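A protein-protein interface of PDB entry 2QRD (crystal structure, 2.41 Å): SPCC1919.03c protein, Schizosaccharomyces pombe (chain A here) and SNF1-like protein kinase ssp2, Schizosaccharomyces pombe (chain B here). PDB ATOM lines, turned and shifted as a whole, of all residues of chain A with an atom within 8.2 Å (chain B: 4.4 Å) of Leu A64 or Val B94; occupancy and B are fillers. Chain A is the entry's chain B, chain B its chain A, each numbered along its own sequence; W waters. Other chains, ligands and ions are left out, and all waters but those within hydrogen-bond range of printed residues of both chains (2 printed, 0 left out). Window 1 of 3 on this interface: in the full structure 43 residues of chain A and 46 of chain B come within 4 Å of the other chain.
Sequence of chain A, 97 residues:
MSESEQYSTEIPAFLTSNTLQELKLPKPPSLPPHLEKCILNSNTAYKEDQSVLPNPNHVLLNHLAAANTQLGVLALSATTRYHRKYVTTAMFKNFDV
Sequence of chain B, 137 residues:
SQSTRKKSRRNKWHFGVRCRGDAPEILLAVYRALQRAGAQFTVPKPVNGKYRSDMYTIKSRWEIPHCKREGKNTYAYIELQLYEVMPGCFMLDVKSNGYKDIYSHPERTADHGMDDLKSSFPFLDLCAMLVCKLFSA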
ATOM      1  N   LEU A  35     -12.790 -32.666  17.449  1.00  0.00           N
ATOM      2  CA  LEU A  35     -13.150 -31.395  16.771  1.00  0.00           C
ATOM      3  C   LEU A  35     -13.667 -30.304  17.711  1.00  0.00           C
ATOM      4  O   LEU A  35     -14.259 -29.305  17.280  1.00  0.00           O
ATOM      5  CB  LEU A  35     -14.186 -31.638  15.659  1.00  0.00           C
ATOM      6  CG  LEU A  35     -13.723 -32.307  14.357  1.00  0.00           C
ATOM      7  CD1 LEU A  35     -14.901 -32.984  13.663  1.00  0.00           C
ATOM      8  CD2 LEU A  35     -13.017 -31.322  13.427  1.00  0.00           C
ATOM      9  N   CYS A  38      -9.538 -26.268  19.136  1.00  0.00           N
ATOM     10  CA  CYS A  38      -8.724 -25.718  18.063  1.00  0.00           C
ATOM     11  C   CYS A  38      -7.406 -25.176  18.635  1.00  0.00           C
ATOM     12  O   CYS A  38      -7.425 -24.475  19.646  1.00  0.00           O
ATOM     13  CB  CYS A  38      -9.533 -24.660  17.298  1.00  0.00           C
ATOM     14  SG  CYS A  38      -8.555 -23.688  16.177  1.00  0.00           S
ATOM     15  N   LEU A  60      -6.477 -33.543  12.070  1.00  0.00           N
ATOM     16  CA  LEU A  60      -7.165 -32.259  11.885  1.00  0.00           C
ATOM     17  C   LEU A  60      -6.442 -31.315  10.922  1.00  0.00           C
ATOM     18  O   LEU A  60      -6.733 -30.107  10.858  1.00  0.00           O
ATOM     19  CB  LEU A  60      -7.396 -31.563  13.228  1.00  0.00           C
ATOM     20  CG  LEU A  60      -8.145 -32.328  14.331  1.00  0.00           C
ATOM     21  CD1 LEU A  60      -8.075 -31.579  15.669  1.00  0.00           C
ATOM     22  CD2 LEU A  60      -9.584 -32.618  13.910  1.00  0.00           C
ATOM     23  N   LEU A  61      -5.495 -31.872  10.187  1.00  0.00           N
ATOM     24  CA  LEU A  61      -4.843 -31.199   9.081  1.00  0.00           C
ATOM     25  C   LEU A  61      -5.826 -30.811   7.948  1.00  0.00           C
ATOM     26  O   LEU A  61      -6.663 -31.610   7.516  1.00  0.00           O
ATOM     27  CB  LEU A  61      -3.698 -32.077   8.558  1.00  0.00           C
ATOM     28  CG  LEU A  61      -2.274 -31.776   9.065  1.00  0.00           C
ATOM     29  CD1 LEU A  61      -2.230 -31.110  10.431  1.00  0.00           C
ATOM     30  CD2 LEU A  61      -1.430 -33.029   9.062  1.00  0.00           C
ATOM     31  N   ASN A  62      -5.707 -29.568   7.495  1.00  0.00           N
ATOM     32  CA  ASN A  62      -6.571 -28.979   6.471  1.00  0.00           C
ATOM     33  C   ASN A  62      -8.077 -29.164   6.674  1.00  0.00           C
ATOM     34  O   ASN A  62      -8.831 -29.356   5.739  1.00  0.00           O
ATOM     35  CB  ASN A  62      -6.064 -29.295   5.049  1.00  0.00           C
ATOM     36  CG  ASN A  62      -4.704 -28.594   4.726  1.00  0.00           C
ATOM     37  OD1 ASN A  62      -3.760 -29.243   4.271  1.00  0.00           O
ATOM     38  ND2 ASN A  62      -4.604 -27.287   4.997  1.00  0.00           N
ATOM     39  N   HIS A  63      -8.487 -29.091   7.937  1.00  0.00           N
ATOM     40  CA  HIS A  63      -9.865 -28.822   8.322  1.00  0.00           C
ATOM     41  C   HIS A  63     -10.013 -27.326   8.536  1.00  0.00           C
ATOM     42  O   HIS A  63      -9.199 -26.689   9.201  1.00  0.00           O
ATOM     43  CB  HIS A  63     -10.223 -29.559   9.622  1.00  0.00           C
ATOM     44  CG  HIS A  63     -10.433 -31.029   9.443  1.00  0.00           C
ATOM     45  ND1 HIS A  63     -11.686 -31.598   9.385  1.00  0.00           N
ATOM     46  CD2 HIS A  63      -9.556 -32.042   9.283  1.00  0.00           C
ATOM     47  CE1 HIS A  63     -11.574 -32.901   9.198  1.00  0.00           C
ATOM     48  NE2 HIS A  63     -10.290 -33.194   9.124  1.00  0.00           N
ATOM     49  N   LEU A  64     -11.066 -26.759   7.963  1.00  0.00           N
ATOM     50  CA  LEU A  64     -11.342 -25.360   8.138  1.00  0.00           C
ATOM     51  C   LEU A  64     -11.688 -25.026   9.617  1.00  0.00           C
ATOM     52  O   LEU A  64     -12.552 -25.683  10.220  1.00  0.00           O
ATOM     53  CB  LEU A  64     -12.486 -24.935   7.195  1.00  0.00           C
ATOM     54  CG  LEU A  64     -13.187 -23.599   7.514  1.00  0.00           C
ATOM     55  CD1 LEU A  64     -12.248 -22.423   7.232  1.00  0.00           C
ATOM     56  CD2 LEU A  64     -14.483 -23.445   6.756  1.00  0.00           C
ATOM     57  N   ALA A  65     -11.026 -24.014  10.179  1.00  0.00           N
ATOM     58  CA  ALA A  65     -11.498 -23.378  11.409  1.00  0.00           C
ATOM     59  C   ALA A  65     -11.952 -21.908  11.148  1.00  0.00           C
ATOM     60  O   ALA A  65     -11.642 -21.331  10.112  1.00  0.00           O
ATOM     61  CB  ALA A  65     -10.439 -23.470  12.536  1.00  0.00           C
ATOM     62  N   ALA A  66     -12.710 -21.326  12.064  1.00  0.00           N
ATOM     63  CA  ALA A  66     -13.382 -20.043  11.814  1.00  0.00           C
ATOM     64  C   ALA A  66     -13.447 -19.334  13.151  1.00  0.00           C
ATOM     65  O   ALA A  66     -13.487 -20.010  14.191  1.00  0.00           O
ATOM     66  CB  ALA A  66     -14.847 -20.250  11.220  1.00  0.00           C
ATOM     67  N   ALA A  67     -13.462 -17.994  13.131  1.00  0.00           N
ATOM     68  CA  ALA A  67     -13.624 -17.161  14.348  1.00  0.00           C
ATOM     69  C   ALA A  67     -14.544 -15.986  14.028  1.00  0.00           C
ATOM     70  O   ALA A  67     -14.537 -15.494  12.871  1.00  0.00           O
ATOM     71  CB  ALA A  67     -12.274 -16.642  14.827  1.00  0.00           C
ATOM     72  N   ALA A  75     -12.537 -14.480   9.321  1.00  0.00           N
ATOM     73  CA  ALA A  75     -11.337 -15.086   9.820  1.00  0.00           C
ATOM     74  C   ALA A  75     -11.426 -16.606   9.613  1.00  0.00           C
ATOM     75  O   ALA A  75     -12.337 -17.252  10.136  1.00  0.00           O
ATOM     76  CB  ALA A  75     -11.145 -14.722  11.311  1.00  0.00           C
ATOM     77  N   LEU A  76     -10.487 -17.147   8.833  1.00  0.00           N
ATOM     78  CA  LEU A  76     -10.474 -18.539   8.398  1.00  0.00           C
ATOM     79  C   LEU A  76      -9.068 -19.095   8.583  1.00  0.00           C
ATOM     80  O   LEU A  76      -8.096 -18.360   8.408  1.00  0.00           O
ATOM     81  CB  LEU A  76     -10.917 -18.660   6.917  1.00  0.00           C
ATOM     82  CG  LEU A  76     -12.269 -18.011   6.546  1.00  0.00           C
ATOM     83  CD1 LEU A  76     -12.544 -18.176   5.112  1.00  0.00           C
ATOM     84  CD2 LEU A  76     -13.480 -18.555   7.367  1.00  0.00           C
ATOM     85  N   SER A  77      -8.952 -20.366   8.979  1.00  0.00           N
ATOM     86  CA  SER A  77      -7.640 -20.983   9.134  1.00  0.00           C
ATOM     87  C   SER A  77      -7.625 -22.450   8.801  1.00  0.00           C
ATOM     88  O   SER A  77      -8.651 -23.118   8.824  1.00  0.00           O
ATOM     89  CB  SER A  77      -7.064 -20.787  10.537  1.00  0.00           C
ATOM     90  OG  SER A  77      -7.945 -21.225  11.563  1.00  0.00           O
ATOM     91  N   ALA A  78      -6.443 -22.947   8.472  1.00  0.00           N
ATOM     92  CA  ALA A  78      -6.250 -24.378   8.369  1.00  0.00           C
ATOM     93  C   ALA A  78      -4.790 -24.683   8.698  1.00  0.00           C
ATOM     94  O   ALA A  78      -3.948 -23.809   8.589  1.00  0.00           O
ATOM     95  CB  ALA A  78      -6.667 -24.896   6.986  1.00  0.00           C
ATOM     96  N   THR A  79      -4.524 -25.901   9.161  1.00  0.00           N
ATOM     97  CA  THR A  79      -3.178 -26.328   9.539  1.00  0.00           C
ATOM     98  C   THR A  79      -2.708 -27.275   8.497  1.00  0.00           C
ATOM     99  O   THR A  79      -3.445 -28.136   8.065  1.00  0.00           O
ATOM    100  CB  THR A  79      -3.135 -27.008  10.938  1.00  0.00           C
ATOM    101  OG1 THR A  79      -3.469 -26.040  11.937  1.00  0.00           O
ATOM    102  CG2 THR A  79      -1.731 -27.538  11.269  1.00  0.00           C
ATOM    103  N   THR A  89      -2.188 -21.218   9.023  1.00  0.00           N
ATOM    104  CA  THR A  89      -2.434 -19.901   8.484  1.00  0.00           C
ATOM    105  C   THR A  89      -3.816 -19.410   8.814  1.00  0.00           C
ATOM    106  O   THR A  89      -4.800 -20.083   8.547  1.00  0.00           O
ATOM    107  CB  THR A  89      -1.987 -19.660   6.997  1.00  0.00           C
ATOM    108  OG1 THR A  89      -3.037 -19.024   6.251  1.00  0.00           O
ATOM    109  CG2 THR A  89      -1.507 -20.857   6.331  1.00  0.00           C
ATOM    110  N   PHE B  15     -13.724 -25.237  14.874  1.00  0.00           N
ATOM    111  CA  PHE B  15     -13.701 -25.946  13.617  1.00  0.00           C
ATOM    112  C   PHE B  15     -15.055 -25.737  12.953  1.00  0.00           C
ATOM    113  O   PHE B  15     -16.077 -25.618  13.639  1.00  0.00           O
ATOM    114  CB  PHE B  15     -13.411 -27.435  13.823  1.00  0.00           C
ATOM    115  CG  PHE B  15     -11.943 -27.757  13.950  1.00  0.00           C
ATOM    116  CD1 PHE B  15     -11.412 -28.207  15.164  1.00  0.00           C
ATOM    117  CD2 PHE B  15     -11.082 -27.601  12.864  1.00  0.00           C
ATOM    118  CE1 PHE B  15     -10.047 -28.505  15.287  1.00  0.00           C
ATOM    119  CE2 PHE B  15      -9.717 -27.890  12.971  1.00  0.00           C
ATOM    120  CZ  PHE B  15      -9.202 -28.336  14.186  1.00  0.00           C
ATOM    121  N   GLY B  16     -15.024 -25.631  11.622  1.00  0.00           N
ATOM    122  CA  GLY B  16     -16.200 -25.600  10.786  1.00  0.00           C
ATOM    123  C   GLY B  16     -16.985 -24.310  10.833  1.00  0.00           C
ATOM    124  O   GLY B  16     -16.460 -23.273  11.224  1.00  0.00           O
ATOM    125  N   ILE B  78     -13.079 -30.969  -1.756  1.00  0.00           N
ATOM    126  CA  ILE B  78     -13.478 -30.531  -0.427  1.00  0.00           C
ATOM    127  C   ILE B  78     -14.606 -31.481   0.048  1.00  0.00           C
ATOM    128  O   ILE B  78     -15.619 -31.673  -0.636  1.00  0.00           O
ATOM    129  CB  ILE B  78     -13.920 -29.017  -0.454  1.00  0.00           C
ATOM    130  CG1 ILE B  78     -12.758 -28.106  -0.884  1.00  0.00           C
ATOM    131  CG2 ILE B  78     -14.506 -28.550   0.902  1.00  0.00           C
ATOM    132  CD1 ILE B  78     -13.116 -26.636  -1.161  1.00  0.00           C
ATOM    133  N   GLU B  79     -14.416 -32.104   1.195  1.00  0.00           N
ATOM    134  CA  GLU B  79     -15.464 -32.939   1.777  1.00  0.00           C
ATOM    135  C   GLU B  79     -16.144 -32.231   2.950  1.00  0.00           C
ATOM    136  O   GLU B  79     -15.487 -31.687   3.836  1.00  0.00           O
ATOM    137  CB  GLU B  79     -14.870 -34.257   2.222  1.00  0.00           C
ATOM    138  CG  GLU B  79     -15.853 -35.192   2.870  1.00  0.00           C
ATOM    139  CD  GLU B  79     -15.173 -36.407   3.487  1.00  0.00           C
ATOM    140  OE1 GLU B  79     -14.096 -36.820   2.972  1.00  0.00           O
ATOM    141  OE2 GLU B  79     -15.716 -36.945   4.489  1.00  0.00           O
ATOM    142  N   LEU B  80     -17.472 -32.230   2.939  1.00  0.00           N
ATOM    143  CA  LEU B  80     -18.256 -31.582   3.988  1.00  0.00           C
ATOM    144  C   LEU B  80     -18.862 -32.639   4.863  1.00  0.00           C
ATOM    145  O   LEU B  80     -19.248 -33.678   4.380  1.00  0.00           O
ATOM    146  CB  LEU B  80     -19.373 -30.730   3.415  1.00  0.00           C
ATOM    147  CG  LEU B  80     -19.146 -29.644   2.351  1.00  0.00           C
ATOM    148  CD1 LEU B  80     -18.259 -28.542   2.845  1.00  0.00           C
ATOM    149  CD2 LEU B  80     -18.668 -30.183   1.023  1.00  0.00           C
ATOM    150  N   LEU B  92     -20.842 -27.722  10.491  1.00  0.00           N
ATOM    151  CA  LEU B  92     -20.457 -28.162   9.171  1.00  0.00           C
ATOM    152  C   LEU B  92     -18.924 -28.213   9.130  1.00  0.00           C
ATOM    153  O   LEU B  92     -18.249 -27.186   9.106  1.00  0.00           O
ATOM    154  CB  LEU B  92     -21.033 -27.236   8.104  1.00  0.00           C
ATOM    155  CG  LEU B  92     -20.800 -27.584   6.623  1.00  0.00           C
ATOM    156  CD1 LEU B  92     -21.502 -28.926   6.256  1.00  0.00           C
ATOM    157  CD2 LEU B  92     -21.300 -26.405   5.772  1.00  0.00           C
ATOM    158  N   ASP B  93     -18.383 -29.423   9.179  1.00  0.00           N
ATOM    159  CA  ASP B  93     -16.953 -29.636   9.072  1.00  0.00           C
ATOM    160  C   ASP B  93     -16.567 -29.640   7.563  1.00  0.00           C
ATOM    161  O   ASP B  93     -17.297 -30.169   6.718  1.00  0.00           O
ATOM    162  CB  ASP B  93     -16.549 -30.915   9.835  1.00  0.00           C
ATOM    163  CG  ASP B  93     -15.051 -31.259   9.700  1.00  0.00           C
ATOM    164  OD1 ASP B  93     -14.180 -30.513  10.253  1.00  0.00           O
ATOM    165  OD2 ASP B  93     -14.752 -32.289   9.042  1.00  0.00           O
ATOM    166  N   VAL B  94     -15.443 -28.994   7.233  1.00  0.00           N
ATOM    167  CA  VAL B  94     -15.045 -28.745   5.844  1.00  0.00           C
ATOM    168  C   VAL B  94     -13.543 -28.999   5.778  1.00  0.00           C
ATOM    169  O   VAL B  94     -12.752 -28.332   6.486  1.00  0.00           O
ATOM    170  CB  VAL B  94     -15.326 -27.271   5.379  1.00  0.00           C
ATOM    171  CG1 VAL B  94     -14.828 -27.050   3.945  1.00  0.00           C
ATOM    172  CG2 VAL B  94     -16.819 -26.890   5.502  1.00  0.00           C
ATOM    173  N   LYS B  95     -13.151 -29.970   4.952  1.00  0.00           N
ATOM    174  CA  LYS B  95     -11.770 -30.390   4.882  1.00  0.00           C
ATOM    175  C   LYS B  95     -11.210 -30.533   3.470  1.00  0.00           C
ATOM    176  O   LYS B  95     -11.904 -30.915   2.522  1.00  0.00           O
ATOM    177  CB  LYS B  95     -11.570 -31.702   5.638  1.00  0.00           C
ATOM    178  CG  LYS B  95     -12.071 -32.926   4.914  1.00  0.00           C
ATOM    179  CD  LYS B  95     -11.390 -34.186   5.392  1.00  0.00           C
ATOM    180  CE  LYS B  95     -12.411 -35.330   5.351  1.00  0.00           C
ATOM    181  NZ  LYS B  95     -11.850 -36.647   4.962  1.00  0.00           N
ATOM    182  N   PHE B 123      -7.546 -23.830  -1.088  1.00  0.00           N
ATOM    183  CA  PHE B 123      -8.557 -24.403  -0.235  1.00  0.00           C
ATOM    184  C   PHE B 123      -9.300 -23.346   0.587  1.00  0.00           C
ATOM    185  O   PHE B 123     -10.528 -23.281   0.512  1.00  0.00           O
ATOM    186  CB  PHE B 123      -7.954 -25.471   0.692  1.00  0.00           C
ATOM    187  CG  PHE B 123      -8.863 -25.860   1.848  1.00  0.00           C
ATOM    188  CD1 PHE B 123     -10.114 -26.442   1.613  1.00  0.00           C
ATOM    189  CD2 PHE B 123      -8.466 -25.631   3.162  1.00  0.00           C
ATOM    190  CE1 PHE B 123     -10.939 -26.820   2.685  1.00  0.00           C
ATOM    191  CE2 PHE B 123      -9.292 -25.984   4.220  1.00  0.00           C
ATOM    192  CZ  PHE B 123     -10.518 -26.583   3.971  1.00  0.00           C
ATOM    193  N   LEU B 124      -8.560 -22.556   1.370  1.00  0.00           N
ATOM    194  CA  LEU B 124      -9.152 -21.504   2.182  1.00  0.00           C
ATOM    195  C   LEU B 124      -9.830 -20.374   1.393  1.00  0.00           C
ATOM    196  O   LEU B 124     -10.727 -19.717   1.927  1.00  0.00           O
ATOM    197  CB  LEU B 124      -8.112 -20.890   3.156  1.00  0.00           C
ATOM    198  CG  LEU B 124      -7.680 -21.687   4.396  1.00  0.00           C
ATOM    199  CD1 LEU B 124      -6.559 -20.954   5.125  1.00  0.00           C
ATOM    200  CD2 LEU B 124      -8.870 -21.931   5.303  1.00  0.00           C
ATOM    201  N   CYS B 127     -13.204 -21.996   0.685  1.00  0.00           N
ATOM    202  CA  CYS B 127     -14.011 -21.999   1.882  1.00  0.00           C
ATOM    203  C   CYS B 127     -14.667 -20.652   2.150  1.00  0.00           C
ATOM    204  O   CYS B 127     -15.781 -20.598   2.674  1.00  0.00           O
ATOM    205  CB  CYS B 127     -13.152 -22.357   3.086  1.00  0.00           C
ATOM    206  SG  CYS B 127     -12.623 -24.077   3.206  1.00  0.00           S
HETATM  207  O   HOH W   1     -14.038 -26.695  17.442  1.00  0.00           O
HETATM  208  O   HOH W   2     -14.124 -28.127   9.578  1.00  0.00           O
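N of Gly B16 lies within hydrogen-bond range of O of Leu A64 (2.8 Å).
The backbone NH (N) of Leu A64 sits at hydrogen-bond distance from the backbone carbonyl oxygen (O) of Val B94 (2.7 Å).
A ring nitrogen (ND1) of His A63 sits at hydrogen-bond distance from the side-chain carboxylate (OD1) of Asp B93 (2.9 Å).
The backbone NH (N) of Thr A89 is in hydrogen-bond range of the backbone carbonyl oxygen (O) of Ala A78 (3.2 Å).
The side-chain sulfur of Cys B127 sits close to the backbone carbonyl oxygen of Phe B123 (3.5 Å).
N of Asn A62 lies within hydrogen-bond range of O of Thr A79, at 2.7 Å.
The side-chain amino group (NZ) of Lys B95 lies within salt-bridge range of the side-chain carboxylate (OE1) of Glu B79 (3.0 Å).
N of Ala A65 sits at hydrogen-bond distance from O of Ser A77 (2.9 Å).
O of Leu A35 touches CD1 of Phe B15, 3.7 Å away.
CD2 of Leu A35 touches OD1 of Asp B93, at 3.5 Å.
Asn A62 touches Lys B95.
Asn A62 touches Phe B123 (O to CZ, 3.7 Å).
His A63 touches Val B94 (CA to O, 3.5 Å).
Phe B15 touches Leu A64 (CD2 to O, 3.6 Å).
O of Gly B16 touches CB of Ala A66 (3.4 Å).
Leu A76 touches Leu B124 (CD1 to O, 3.98 Å).
CB of Ala A78 touches CE2 of Phe B123, at 3.97 Å.
Leu B124 touches Ala A78.
Of the printed residues of chain B, Leu A60 touches Phe B15 (3.7 Å).
Leu A64 touches four residues of chain B.
Ala A67 touches none of the printed residues of chain B.
Printed residues of chain B within 4 Å of Ser A77: Leu B124.
Of the printed residues of chain A, Phe B15 touches Leu A35 (3.7 Å), Leu A60 (3.7 Å), His A63 (3.8 Å) and Leu A64 (3.6 Å).
Leu B92 touches none of the printed residues of chain A.
Of chain A, only Leu A35 and His A63 come within 4 Å of Asp B93.
Val B94 touches two residues of chain A.
The nearest printed residue of chain B that does not touch Leu A64 is Phe B123 (4.03 Å).
The nearest residue of chain A that does not touch Val B94 is Asn A62 (4.1 Å).
The nearest printed residue of chain B that does not touch Ala A78 is Phe B15 (6.7 Å).
Of the 12 printed residues of chain B, 7 touch a printed residue of chain A.
Hydrophobic or aromatic side chains of chain B that line the printed part of chain A: Phe B15, Phe B123 and Leu B124.
Along chain B the printed residues that touch a printed residue of chain A span positions 15 to 124.
Of the 16 printed residues of chain A, 10 touch a printed residue of chain B.
Among the printed residues, 19 pairs touch across the chains.
Among the printed residues, no Asp or Glu carboxylate lies within 4 Å of a Lys or Arg side-chain nitrogen of the other chain.
Water W2 lies within hydrogen-bond range of OD1 of Asp B93, N of Val B94, O of Leu A64 and N of Gly B16.
Water W1 lies within hydrogen-bond range of O of Leu A35 (2.6 Å) and N of Phe B15 (3.0 Å).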
